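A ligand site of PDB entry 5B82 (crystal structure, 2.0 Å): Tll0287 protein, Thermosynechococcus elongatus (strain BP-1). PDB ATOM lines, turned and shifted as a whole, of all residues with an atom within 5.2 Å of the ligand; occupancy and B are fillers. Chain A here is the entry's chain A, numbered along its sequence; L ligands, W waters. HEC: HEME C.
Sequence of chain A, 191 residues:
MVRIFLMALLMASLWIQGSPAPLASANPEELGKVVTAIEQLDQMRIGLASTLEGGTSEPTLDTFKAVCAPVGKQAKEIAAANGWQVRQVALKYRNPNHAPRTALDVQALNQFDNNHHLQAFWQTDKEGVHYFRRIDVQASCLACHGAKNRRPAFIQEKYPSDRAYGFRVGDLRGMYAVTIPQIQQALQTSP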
ATOM      1  N   ARG A  45      19.613  32.083  -6.218  1.00  0.00           N
ATOM      2  CA  ARG A  45      18.562  31.324  -6.896  1.00  0.00           C
ATOM      3  C   ARG A  45      17.205  31.556  -6.256  1.00  0.00           C
ATOM      4  O   ARG A  45      16.210  31.837  -6.945  1.00  0.00           O
ATOM      5  CB  ARG A  45      18.840  29.818  -6.922  1.00  0.00           C
ATOM      6  CG  ARG A  45      17.988  29.093  -7.968  1.00  0.00           C
ATOM      7  CD  ARG A  45      17.703  27.647  -7.583  1.00  0.00           C
ATOM      8  NE  ARG A  45      18.914  26.971  -7.131  1.00  0.00           N
ATOM      9  CZ  ARG A  45      19.822  26.425  -7.929  1.00  0.00           C
ATOM     10  NH1 ARG A  45      19.657  26.471  -9.242  1.00  0.00           N
ATOM     11  NH2 ARG A  45      20.892  25.844  -7.406  1.00  0.00           N
ATOM     12  N   ILE A  46      17.163  31.447  -4.934  1.00  0.00           N
ATOM     13  CA  ILE A  46      15.906  31.632  -4.207  1.00  0.00           C
ATOM     14  C   ILE A  46      15.287  32.990  -4.534  1.00  0.00           C
ATOM     15  O   ILE A  46      14.070  33.109  -4.741  1.00  0.00           O
ATOM     16  CB  ILE A  46      16.134  31.473  -2.702  1.00  0.00           C
ATOM     17  CG1 ILE A  46      16.290  29.990  -2.367  1.00  0.00           C
ATOM     18  CG2 ILE A  46      14.980  32.074  -1.904  1.00  0.00           C
ATOM     19  CD1 ILE A  46      16.916  29.722  -1.021  1.00  0.00           C
ATOM     20  N   ALA A  49      13.787  33.009  -8.116  1.00  0.00           N
ATOM     21  CA  ALA A  49      12.549  32.227  -8.169  1.00  0.00           C
ATOM     22  C   ALA A  49      11.405  32.840  -7.359  1.00  0.00           C
ATOM     23  O   ALA A  49      10.252  32.539  -7.624  1.00  0.00           O
ATOM     24  CB  ALA A  49      12.808  30.795  -7.722  1.00  0.00           C
ATOM     25  N   LEU A  52       7.714  33.927  -8.431  1.00  0.00           N
ATOM     26  CA  LEU A  52       6.828  32.957  -9.072  1.00  0.00           C
ATOM     27  C   LEU A  52       6.029  32.160  -8.036  1.00  0.00           C
ATOM     28  O   LEU A  52       6.554  31.812  -6.980  1.00  0.00           O
ATOM     29  CB  LEU A  52       7.641  32.012  -9.967  1.00  0.00           C
ATOM     30  CG  LEU A  52       8.828  32.624 -10.721  1.00  0.00           C
ATOM     31  CD1 LEU A  52       9.630  31.558 -11.455  1.00  0.00           C
ATOM     32  CD2 LEU A  52       8.390  33.712 -11.688  1.00  0.00           C
ATOM     33  N   ASP A  62       5.917  34.762 -17.057  1.00  0.00           N
ATOM     34  CA  ASP A  62       6.962  34.838 -16.047  1.00  0.00           C
ATOM     35  C   ASP A  62       7.869  33.619 -16.007  1.00  0.00           C
ATOM     36  O   ASP A  62       9.015  33.709 -15.570  1.00  0.00           O
ATOM     37  CB  ASP A  62       6.361  35.065 -14.659  1.00  0.00           C
ATOM     38  CG  ASP A  62       5.712  36.432 -14.534  1.00  0.00           C
ATOM     39  OD1 ASP A  62       6.087  37.346 -15.293  1.00  0.00           O
ATOM     40  OD2 ASP A  62       4.811  36.576 -13.676  1.00  0.00           O
ATOM     41  N   THR A  63       7.385  32.470 -16.472  1.00  0.00           N
ATOM     42  CA  THR A  63       8.205  31.263 -16.457  1.00  0.00           C
ATOM     43  C   THR A  63       9.353  31.296 -17.468  1.00  0.00           C
ATOM     44  O   THR A  63      10.281  30.505 -17.369  1.00  0.00           O
ATOM     45  CB  THR A  63       7.374  29.980 -16.640  1.00  0.00           C
ATOM     46  OG1 THR A  63       6.719  30.004 -17.913  1.00  0.00           O
ATOM     47  CG2 THR A  63       6.341  29.837 -15.535  1.00  0.00           C
ATOM     48  N   LYS A  65      11.387  33.549 -17.479  1.00  0.00           N
ATOM     49  CA  LYS A  65      12.426  34.238 -16.714  1.00  0.00           C
ATOM     50  C   LYS A  65      13.595  33.301 -16.438  1.00  0.00           C
ATOM     51  O   LYS A  65      13.402  32.130 -16.143  1.00  0.00           O
ATOM     52  CB  LYS A  65      11.829  34.728 -15.396  1.00  0.00           C
ATOM     53  CG  LYS A  65      12.787  35.336 -14.398  1.00  0.00           C
ATOM     54  CD  LYS A  65      12.070  35.634 -13.075  1.00  0.00           C
ATOM     55  CE  LYS A  65      12.953  36.394 -12.094  1.00  0.00           C
ATOM     56  NZ  LYS A  65      12.270  36.649 -10.786  1.00  0.00           N
ATOM     57  N   VAL A  67      16.195  31.711 -14.226  1.00  0.00           N
ATOM     58  CA  VAL A  67      16.286  31.494 -12.796  1.00  0.00           C
ATOM     59  C   VAL A  67      17.551  30.694 -12.479  1.00  0.00           C
ATOM     60  O   VAL A  67      18.409  31.158 -11.737  1.00  0.00           O
ATOM     61  CB  VAL A  67      15.022  30.803 -12.251  1.00  0.00           C
ATOM     62  CG1 VAL A  67      15.240  30.260 -10.847  1.00  0.00           C
ATOM     63  CG2 VAL A  67      13.819  31.777 -12.295  1.00  0.00           C
ATOM     64  N   CYS A  68      17.663  29.507 -13.061  1.00  0.00           N
ATOM     65  CA  CYS A  68      18.754  28.599 -12.697  1.00  0.00           C
ATOM     66  C   CYS A  68      19.997  28.694 -13.600  1.00  0.00           C
ATOM     67  O   CYS A  68      21.107  28.437 -13.145  1.00  0.00           O
ATOM     68  CB  CYS A  68      18.239  27.169 -12.612  1.00  0.00           C
ATOM     69  SG  CYS A  68      17.075  26.851 -11.250  1.00  0.00           S
ATOM     70  N   ALA A  69      19.823  29.078 -14.866  1.00  0.00           N
ATOM     71  CA  ALA A  69      20.978  29.264 -15.760  1.00  0.00           C
ATOM     72  C   ALA A  69      22.045  30.236 -15.212  1.00  0.00           C
ATOM     73  O   ALA A  69      23.243  29.906 -15.204  1.00  0.00           O
ATOM     74  CB  ALA A  69      20.529  29.667 -17.169  1.00  0.00           C
ATOM     75  N   GLY A  72      24.292  28.517 -12.685  1.00  0.00           N
ATOM     76  CA  GLY A  72      25.365  27.726 -13.286  1.00  0.00           C
ATOM     77  C   GLY A  72      26.484  28.603 -13.825  1.00  0.00           C
ATOM     78  O   GLY A  72      27.686  28.289 -13.664  1.00  0.00           O
ATOM     79  N   GLN A  88      26.795  22.113  -9.625  1.00  0.00           N
ATOM     80  CA  GLN A  88      25.541  21.589  -9.101  1.00  0.00           C
ATOM     81  C   GLN A  88      25.444  20.134  -9.495  1.00  0.00           C
ATOM     82  O   GLN A  88      25.841  19.753 -10.601  1.00  0.00           O
ATOM     83  CB  GLN A  88      24.363  22.360  -9.671  1.00  0.00           C
ATOM     84  CG  GLN A  88      24.324  23.814  -9.242  1.00  0.00           C
ATOM     85  CD  GLN A  88      23.350  24.622 -10.067  1.00  0.00           C
ATOM     86  OE1 GLN A  88      22.217  24.879  -9.652  1.00  0.00           O
ATOM     87  NE2 GLN A  88      23.771  25.020 -11.263  1.00  0.00           N
ATOM     88  N   ALA A  90      22.717  16.713  -9.222  1.00  0.00           N
ATOM     89  CA  ALA A  90      21.406  16.178  -8.843  1.00  0.00           C
ATOM     90  C   ALA A  90      21.163  14.819  -9.495  1.00  0.00           C
ATOM     91  O   ALA A  90      21.555  14.586 -10.640  1.00  0.00           O
ATOM     92  CB  ALA A  90      20.292  17.159  -9.218  1.00  0.00           C
ATOM     93  N   LYS A  92      18.168  13.769 -10.239  1.00  0.00           N
ATOM     94  CA  LYS A  92      17.218  14.139 -11.275  1.00  0.00           C
ATOM     95  C   LYS A  92      17.624  15.503 -11.815  1.00  0.00           C
ATOM     96  O   LYS A  92      17.228  16.543 -11.271  1.00  0.00           O
ATOM     97  CB  LYS A  92      15.790  14.207 -10.702  1.00  0.00           C
ATOM     98  CG  LYS A  92      15.357  12.913 -10.024  1.00  0.00           C
ATOM     99  CD  LYS A  92      14.116  13.107  -9.165  1.00  0.00           C
ATOM    100  CE  LYS A  92      12.876  13.403 -10.003  1.00  0.00           C
ATOM    101  NZ  LYS A  92      11.660  13.483  -9.143  1.00  0.00           N
ATOM    102  N   TYR A  93      18.435  15.496 -12.869  1.00  0.00           N
ATOM    103  CA  TYR A  93      19.026  16.714 -13.408  1.00  0.00           C
ATOM    104  C   TYR A  93      18.375  17.161 -14.707  1.00  0.00           C
ATOM    105  O   TYR A  93      17.816  16.362 -15.443  1.00  0.00           O
ATOM    106  CB  TYR A  93      20.529  16.514 -13.641  1.00  0.00           C
ATOM    107  CG  TYR A  93      20.816  15.260 -14.423  1.00  0.00           C
ATOM    108  CD1 TYR A  93      20.851  15.280 -15.814  1.00  0.00           C
ATOM    109  CD2 TYR A  93      21.023  14.048 -13.793  1.00  0.00           C
ATOM    110  CE1 TYR A  93      21.099  14.134 -16.545  1.00  0.00           C
ATOM    111  CE2 TYR A  93      21.274  12.905 -14.494  1.00  0.00           C
ATOM    112  CZ  TYR A  93      21.309  12.948 -15.876  1.00  0.00           C
ATOM    113  OH  TYR A  93      21.561  11.798 -16.570  1.00  0.00           O
ATOM    114  N   ARG A  94      18.469  18.461 -14.971  1.00  0.00           N
ATOM    115  CA  ARG A  94      17.961  19.041 -16.195  1.00  0.00           C
ATOM    116  C   ARG A  94      19.103  19.182 -17.185  1.00  0.00           C
ATOM    117  O   ARG A  94      19.007  18.772 -18.328  1.00  0.00           O
ATOM    118  CB  ARG A  94      17.332  20.398 -15.887  1.00  0.00           C
ATOM    119  CG  ARG A  94      16.824  21.161 -17.089  1.00  0.00           C
ATOM    120  CD  ARG A  94      15.645  22.009 -16.649  1.00  0.00           C
ATOM    121  NE  ARG A  94      14.499  21.161 -16.328  1.00  0.00           N
ATOM    122  CZ  ARG A  94      13.384  21.583 -15.730  1.00  0.00           C
ATOM    123  NH1 ARG A  94      13.256  22.850 -15.362  1.00  0.00           N
ATOM    124  NH2 ARG A  94      12.406  20.728 -15.497  1.00  0.00           N
ATOM    125  N   ASN A  95      20.198  19.776 -16.708  1.00  0.00           N
ATOM    126  CA  ASN A  95      21.401  19.918 -17.508  1.00  0.00           C
ATOM    127  C   ASN A  95      22.286  18.688 -17.298  1.00  0.00           C
ATOM    128  O   ASN A  95      22.652  18.373 -16.158  1.00  0.00           O
ATOM    129  CB  ASN A  95      22.125  21.204 -17.095  1.00  0.00           C
ATOM    130  CG  ASN A  95      23.358  21.496 -17.933  1.00  0.00           C
ATOM    131  OD1 ASN A  95      24.071  20.594 -18.354  1.00  0.00           O
ATOM    132  ND2 ASN A  95      23.612  22.775 -18.158  1.00  0.00           N
ATOM    133  N   HIS A  98      25.182  18.206 -14.828  1.00  0.00           N
ATOM    134  CA  HIS A  98      24.916  18.186 -13.408  1.00  0.00           C
ATOM    135  C   HIS A  98      24.609  16.779 -12.872  1.00  0.00           C
ATOM    136  O   HIS A  98      24.090  16.630 -11.779  1.00  0.00           O
ATOM    137  CB  HIS A  98      23.759  19.153 -13.103  1.00  0.00           C
ATOM    138  CG  HIS A  98      24.062  20.572 -13.475  1.00  0.00           C
ATOM    139  ND1 HIS A  98      23.077  21.505 -13.752  1.00  0.00           N
ATOM    140  CD2 HIS A  98      25.238  21.226 -13.607  1.00  0.00           C
ATOM    141  CE1 HIS A  98      23.646  22.659 -14.047  1.00  0.00           C
ATOM    142  NE2 HIS A  98      24.952  22.519 -13.963  1.00  0.00           N
ATOM    143  N   ILE A 135      20.444  21.295  -1.577  1.00  0.00           N
ATOM    144  CA  ILE A 135      19.459  22.177  -2.179  1.00  0.00           C
ATOM    145  C   ILE A 135      18.086  21.544  -1.985  1.00  0.00           C
ATOM    146  O   ILE A 135      17.860  20.414  -2.436  1.00  0.00           O
ATOM    147  CB  ILE A 135      19.702  22.353  -3.684  1.00  0.00           C
ATOM    148  CG1 ILE A 135      21.070  22.974  -3.930  1.00  0.00           C
ATOM    149  CG2 ILE A 135      18.611  23.232  -4.310  1.00  0.00           C
ATOM    150  CD1 ILE A 135      21.602  22.776  -5.341  1.00  0.00           C
ATOM    151  N   ASP A 136      17.178  22.241  -1.320  1.00  0.00           N
ATOM    152  CA  ASP A 136      15.843  21.707  -1.130  1.00  0.00           C
ATOM    153  C   ASP A 136      14.855  22.369  -2.093  1.00  0.00           C
ATOM    154  O   ASP A 136      15.140  23.410  -2.670  1.00  0.00           O
ATOM    155  CB  ASP A 136      15.381  21.864   0.318  1.00  0.00           C
ATOM    156  CG  ASP A 136      16.130  20.930   1.273  1.00  0.00           C
ATOM    157  OD1 ASP A 136      16.517  19.809   0.861  1.00  0.00           O
ATOM    158  OD2 ASP A 136      16.310  21.301   2.456  1.00  0.00           O
ATOM    159  N   VAL A 137      13.697  21.752  -2.244  1.00  0.00           N
ATOM    160  CA  VAL A 137      12.669  22.286  -3.133  1.00  0.00           C
ATOM    161  C   VAL A 137      11.720  23.197  -2.357  1.00  0.00           C
ATOM    162  O   VAL A 137      11.134  22.757  -1.369  1.00  0.00           O
ATOM    163  CB  VAL A 137      11.858  21.134  -3.758  1.00  0.00           C
ATOM    164  CG1 VAL A 137      10.705  21.689  -4.577  1.00  0.00           C
ATOM    165  CG2 VAL A 137      12.760  20.253  -4.612  1.00  0.00           C
ATOM    166  N   GLN A 138      11.585  24.451  -2.786  1.00  0.00           N
ATOM    167  CA  GLN A 138      10.514  25.329  -2.283  1.00  0.00           C
ATOM    168  C   GLN A 138       9.357  25.421  -3.279  1.00  0.00           C
ATOM    169  O   GLN A 138       9.454  24.916  -4.399  1.00  0.00           O
ATOM    170  CB  GLN A 138      11.020  26.752  -1.987  1.00  0.00           C
ATOM    171  CG  GLN A 138      11.980  26.838  -0.809  1.00  0.00           C
ATOM    172  CD  GLN A 138      13.405  26.653  -1.231  1.00  0.00           C
ATOM    173  OE1 GLN A 138      13.816  27.130  -2.282  1.00  0.00           O
ATOM    174  NE2 GLN A 138      14.186  25.932  -0.421  1.00  0.00           N
ATOM    175  N   SER A 140       8.099  27.875  -5.063  1.00  0.00           N
ATOM    176  CA  SER A 140       8.355  28.610  -6.300  1.00  0.00           C
ATOM    177  C   SER A 140       8.953  27.691  -7.364  1.00  0.00           C
ATOM    178  O   SER A 140       8.589  27.753  -8.537  1.00  0.00           O
ATOM    179  CB  SER A 140       9.309  29.772  -6.020  1.00  0.00           C
ATOM    180  OG  SER A 140      10.528  29.310  -5.449  1.00  0.00           O
ATOM    181  N   CYS A 141       9.840  26.802  -6.928  1.00  0.00           N
ATOM    182  CA  CYS A 141      10.568  25.908  -7.824  1.00  0.00           C
ATOM    183  C   CYS A 141       9.620  25.045  -8.650  1.00  0.00           C
ATOM    184  O   CYS A 141       9.914  24.694  -9.803  1.00  0.00           O
ATOM    185  CB  CYS A 141      11.512  25.018  -7.019  1.00  0.00           C
ATOM    186  SG  CYS A 141      12.380  25.896  -5.705  1.00  0.00           S
ATOM    187  N   ALA A 143       7.213  25.788 -10.243  1.00  0.00           N
ATOM    188  CA  ALA A 143       6.864  26.406 -11.510  1.00  0.00           C
ATOM    189  C   ALA A 143       7.545  25.714 -12.694  1.00  0.00           C
ATOM    190  O   ALA A 143       6.984  25.651 -13.780  1.00  0.00           O
ATOM    191  CB  ALA A 143       7.208  27.890 -11.505  1.00  0.00           C
ATOM    192  N   CYS A 144       8.757  25.185 -12.476  1.00  0.00           N
ATOM    193  CA  CYS A 144       9.527  24.607 -13.586  1.00  0.00           C
ATOM    194  C   CYS A 144      10.057  23.201 -13.285  1.00  0.00           C
ATOM    195  O   CYS A 144      10.524  22.503 -14.186  1.00  0.00           O
ATOM    196  CB  CYS A 144      10.714  25.502 -13.961  1.00  0.00           C
ATOM    197  SG  CYS A 144      10.317  27.208 -14.385  1.00  0.00           S
ATOM    198  N   HIS A 145       9.984  22.811 -12.022  1.00  0.00           N
ATOM    199  CA  HIS A 145      10.410  21.487 -11.581  1.00  0.00           C
ATOM    200  C   HIS A 145       9.257  20.725 -10.931  1.00  0.00           C
ATOM    201  O   HIS A 145       9.474  19.709 -10.267  1.00  0.00           O
ATOM    202  CB  HIS A 145      11.557  21.609 -10.589  1.00  0.00           C
ATOM    203  CG  HIS A 145      12.797  22.254 -11.149  1.00  0.00           C
ATOM    204  ND1 HIS A 145      13.583  21.635 -12.106  1.00  0.00           N
ATOM    205  CD2 HIS A 145      13.411  23.422 -10.854  1.00  0.00           C
ATOM    206  CE1 HIS A 145      14.615  22.406 -12.380  1.00  0.00           C
ATOM    207  NE2 HIS A 145      14.546  23.491 -11.636  1.00  0.00           N
ATOM    208  N   PRO A 152       7.348  24.733 -18.567  1.00  0.00           N
ATOM    209  CA  PRO A 152       7.351  25.801 -19.569  1.00  0.00           C
ATOM    210  C   PRO A 152       7.901  25.317 -20.921  1.00  0.00           C
ATOM    211  O   PRO A 152       8.810  24.497 -20.945  1.00  0.00           O
ATOM    212  CB  PRO A 152       8.285  26.841 -18.962  1.00  0.00           C
ATOM    213  CG  PRO A 152       8.177  26.606 -17.493  1.00  0.00           C
ATOM    214  CD  PRO A 152       8.018  25.130 -17.324  1.00  0.00           C
ATOM    215  N   ILE A 155      11.660  24.411 -22.125  1.00  0.00           N
ATOM    216  CA  ILE A 155      12.383  23.432 -21.322  1.00  0.00           C
ATOM    217  C   ILE A 155      12.632  22.119 -22.059  1.00  0.00           C
ATOM    218  O   ILE A 155      13.766  21.650 -22.151  1.00  0.00           O
ATOM    219  CB  ILE A 155      11.661  23.122 -19.994  1.00  0.00           C
ATOM    220  CG1 ILE A 155      11.537  24.382 -19.135  1.00  0.00           C
ATOM    221  CG2 ILE A 155      12.402  22.043 -19.217  1.00  0.00           C
ATOM    222  CD1 ILE A 155      12.839  24.831 -18.506  1.00  0.00           C
ATOM    223  N   TYR A 159      16.167  20.790 -23.236  1.00  0.00           N
ATOM    224  CA  TYR A 159      16.637  19.717 -22.367  1.00  0.00           C
ATOM    225  C   TYR A 159      15.866  18.418 -22.638  1.00  0.00           C
ATOM    226  O   TYR A 159      14.995  18.040 -21.849  1.00  0.00           O
ATOM    227  CB  TYR A 159      16.477  20.117 -20.900  1.00  0.00           C
ATOM    228  CG  TYR A 159      17.192  21.408 -20.537  1.00  0.00           C
ATOM    229  CD1 TYR A 159      18.526  21.405 -20.144  1.00  0.00           C
ATOM    230  CD2 TYR A 159      16.538  22.626 -20.607  1.00  0.00           C
ATOM    231  CE1 TYR A 159      19.178  22.585 -19.827  1.00  0.00           C
ATOM    232  CE2 TYR A 159      17.176  23.803 -20.292  1.00  0.00           C
ATOM    233  CZ  TYR A 159      18.492  23.784 -19.900  1.00  0.00           C
ATOM    234  OH  TYR A 159      19.107  24.967 -19.590  1.00  0.00           O
ATOM    235  N   ALA A 164      14.406  16.648 -14.132  1.00  0.00           N
ATOM    236  CA  ALA A 164      14.205  17.544 -12.992  1.00  0.00           C
ATOM    237  C   ALA A 164      12.755  17.997 -12.812  1.00  0.00           C
ATOM    238  O   ALA A 164      12.472  19.203 -12.794  1.00  0.00           O
ATOM    239  CB  ALA A 164      15.145  18.750 -13.097  1.00  0.00           C
ATOM    240  N   ARG A 173      16.431  18.398  -3.743  1.00  0.00           N
ATOM    241  CA  ARG A 173      16.569  18.751  -5.144  1.00  0.00           C
ATOM    242  C   ARG A 173      17.894  18.271  -5.741  1.00  0.00           C
ATOM    243  O   ARG A 173      17.958  17.834  -6.891  1.00  0.00           O
ATOM    244  CB  ARG A 173      16.463  20.272  -5.322  1.00  0.00           C
ATOM    245  CG  ARG A 173      16.783  20.757  -6.718  1.00  0.00           C
ATOM    246  CD  ARG A 173      15.677  20.388  -7.713  1.00  0.00           C
ATOM    247  NE  ARG A 173      16.023  20.848  -9.052  1.00  0.00           N
ATOM    248  CZ  ARG A 173      16.724  20.138  -9.937  1.00  0.00           C
ATOM    249  NH1 ARG A 173      17.138  18.918  -9.619  1.00  0.00           N
ATOM    250  NH2 ARG A 173      16.998  20.639 -11.136  1.00  0.00           N
HETATM  251 FE   HEC L   1      15.842  25.137 -11.485  1.00  0.00          FE
HETATM  252  CHA HEC L   1      18.404  23.597 -13.101  1.00  0.00           C
HETATM  253  CHB HEC L   1      17.046  23.848  -8.467  1.00  0.00           C
HETATM  254  CHC HEC L   1      13.469  26.842  -9.751  1.00  0.00           C
HETATM  255  CHD HEC L   1      14.407  26.088 -14.462  1.00  0.00           C
HETATM  256  NA  HEC L   1      17.392  23.894 -10.889  1.00  0.00           N
HETATM  257  C1A HEC L   1      18.407  23.487 -11.729  1.00  0.00           C
HETATM  258  C2A HEC L   1      19.464  22.911 -10.923  1.00  0.00           C
HETATM  259  C3A HEC L   1      19.080  22.991  -9.649  1.00  0.00           C
HETATM  260  C4A HEC L   1      17.770  23.598  -9.608  1.00  0.00           C
HETATM  261  CMA HEC L   1      19.842  22.506  -8.407  1.00  0.00           C
HETATM  262  CAA HEC L   1      20.802  22.330 -11.453  1.00  0.00           C
HETATM  263  CBA HEC L   1      20.778  20.802 -11.535  1.00  0.00           C
HETATM  264  CGA HEC L   1      20.093  20.355 -12.797  1.00  0.00           C
HETATM  265  O1A HEC L   1      19.026  19.696 -12.704  1.00  0.00           O
HETATM  266  O2A HEC L   1      20.582  20.686 -13.909  1.00  0.00           O
HETATM  267  NB  HEC L   1      15.357  25.279  -9.496  1.00  0.00           N
HETATM  268  C1B HEC L   1      15.994  24.730  -8.403  1.00  0.00           C
HETATM  269  C2B HEC L   1      15.374  25.229  -7.198  1.00  0.00           C
HETATM  270  C3B HEC L   1      14.389  26.048  -7.556  1.00  0.00           C
HETATM  271  C4B HEC L   1      14.357  26.108  -9.002  1.00  0.00           C
HETATM  272  CMB HEC L   1      15.768  24.826  -5.757  1.00  0.00           C
HETATM  273  CAB HEC L   1      13.439  26.821  -6.608  1.00  0.00           C
HETATM  274  CBB HEC L   1      14.219  27.885  -5.789  1.00  0.00           C
HETATM  275  NC  HEC L   1      14.215  26.226 -12.014  1.00  0.00           N
HETATM  276  C1C HEC L   1      13.401  26.891 -11.135  1.00  0.00           C
HETATM  277  C2C HEC L   1      12.555  27.775 -11.897  1.00  0.00           C
HETATM  278  C3C HEC L   1      12.712  27.477 -13.198  1.00  0.00           C
HETATM  279  C4C HEC L   1      13.829  26.555 -13.291  1.00  0.00           C
HETATM  280  CMC HEC L   1      11.353  28.538 -11.273  1.00  0.00           C
HETATM  281  CAC HEC L   1      11.932  28.062 -14.413  1.00  0.00           C
HETATM  282  CBC HEC L   1      12.005  29.609 -14.551  1.00  0.00           C
HETATM  283  ND  HEC L   1      16.273  24.835 -13.456  1.00  0.00           N
HETATM  284  C1D HEC L   1      15.626  25.450 -14.527  1.00  0.00           C
HETATM  285  C2D HEC L   1      16.427  25.280 -15.721  1.00  0.00           C
HETATM  286  C3D HEC L   1      17.662  24.498 -15.275  1.00  0.00           C
HETATM  287  C4D HEC L   1      17.482  24.266 -13.868  1.00  0.00           C
HETATM  288  CMD HEC L   1      16.117  25.792 -17.147  1.00  0.00           C
HETATM  289  CAD HEC L   1      18.868  24.068 -16.135  1.00  0.00           C
HETATM  290  CBD HEC L   1      19.850  25.228 -16.052  1.00  0.00           C
HETATM  291  CGD HEC L   1      21.179  24.886 -16.685  1.00  0.00           C
HETATM  292  O1D HEC L   1      21.227  24.635 -17.906  1.00  0.00           O
HETATM  293  O2D HEC L   1      22.190  24.860 -15.948  1.00  0.00           O
HETATM  294  O   HOH W   1      13.932  29.025 -17.248  1.00  0.00           O
HETATM  295  O   HOH W   2      16.228  25.939  -2.730  1.00  0.00           O
HETATM  296  O   HOH W   3      22.231  25.884 -13.529  1.00  0.00           O
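Water W3 lies within hydrogen-bond range of an oxygen (O2D) of the ligand (2.6 Å), the backbone carbonyl oxygen of Cys 68 (2.8 Å), the side-chain amide nitrogen of Gln 88 (2.9 Å) and the backbone NH of Gly 72 (3.4 Å).
Water W2 lies within hydrogen-bond range of OE1 of Gln 138 (2.7 Å) and O of Asp 136 (2.8 Å).
Arg 45 touches the ligand (CD to C2B, 3.4 Å).
Ala 49 touches the ligand.
Leu 52 touches the ligand (CD1 to CMC, 3.5 Å).
Thr 63 touches the ligand (O to CBC, 3.4 Å).
Lys 65 touches the ligand.
CG2 of Val 67 touches CBC of the ligand (3.6 Å).
OE1 of Gln 88 touches CAA of the ligand, at 3.4 Å.
O of Lys 92 touches O1A of the ligand, 3.9 Å away.
Tyr 93 touches the ligand (CA to O1A, 3.1 Å).
Ile 135 touches the ligand.
Asp 136 touches the ligand.
Gln 138 touches the ligand (OE1 to CBB, 3.6 Å).
O of Ser 140 touches CMC of the ligand (3.97 Å).
CD1 of Ile 155 touches CMD of the ligand, 3.7 Å away.
Hydrophobic or aromatic side chains within 4 Å of the ligand: Ala 49, Leu 52, Val 67, Tyr 93, His 98, Ile 135, His 145, Ile 155 and Tyr 159.
Of the 32 residues printed, 23 come within 4 Å of the ligand.
SG of Cys 141 is covalently linked to CAB of the ligand (1.7 Å).
The side-chain sulfur of Cys 144 is bonded to a carbon (CAC) of the ligand, at 1.8 Å.
An iron atom (FE) of the ligand is bound by a ring nitrogen (NE2) of His 145, at 2.1 Å.
The side-chain sulfur of Cys 68 is bound to an iron atom (FE) of the ligand (2.1 Å).
O2A of the ligand sits at hydrogen-bond distance from ND1 of His 98.
The backbone NH of Arg 94 sits at hydrogen-bond distance from an oxygen (O1A) of the ligand, 2.6 Å away.
O1D of the ligand sits at hydrogen-bond distance from OH of Tyr 159, 2.7 Å away.
The guanidinium group of Arg 173 is in salt-bridge range of an oxygen (O1A) of the ligand, 2.7 Å away.
An oxygen (O2A) of the ligand is in hydrogen-bond range of the backbone NH (N) of Asn 95.
An oxygen (O1D) of the ligand sits at hydrogen-bond distance from the side-chain amide nitrogen (ND2) of Asn 95 (3.0 Å).
The backbone NH (N) of Gln 138 lies within hydrogen-bond range of the side-chain sulfur (SG) of Cys 141.
The backbone carbonyl oxygen (O) of Cys 144 lies within hydrogen-bond range of the guanidinium group (NH2) of Arg 94, at 2.9 Å.
NH1 of Arg 94 sits close to ND1 of His 145, 3.5 Å away.
The backbone carbonyl oxygen of Ala 164 is in hydrogen-bond range of a ring nitrogen (ND1) of His 145.
SG of Cys 68 sits close to NH1 of Arg 45 (3.3 Å).
The backbone NH of Arg 173 lies within hydrogen-bond range of the backbone carbonyl oxygen of Ile 135.
The backbone carbonyl oxygen (O) of Lys 92 is in hydrogen-bond range of the guanidinium group (NH1) of Arg 173 (2.9 Å).
The guanidinium group (NH2) of Arg 45 is in hydrogen-bond range of the side-chain amide oxygen (OE1) of Gln 88 (2.8 Å).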
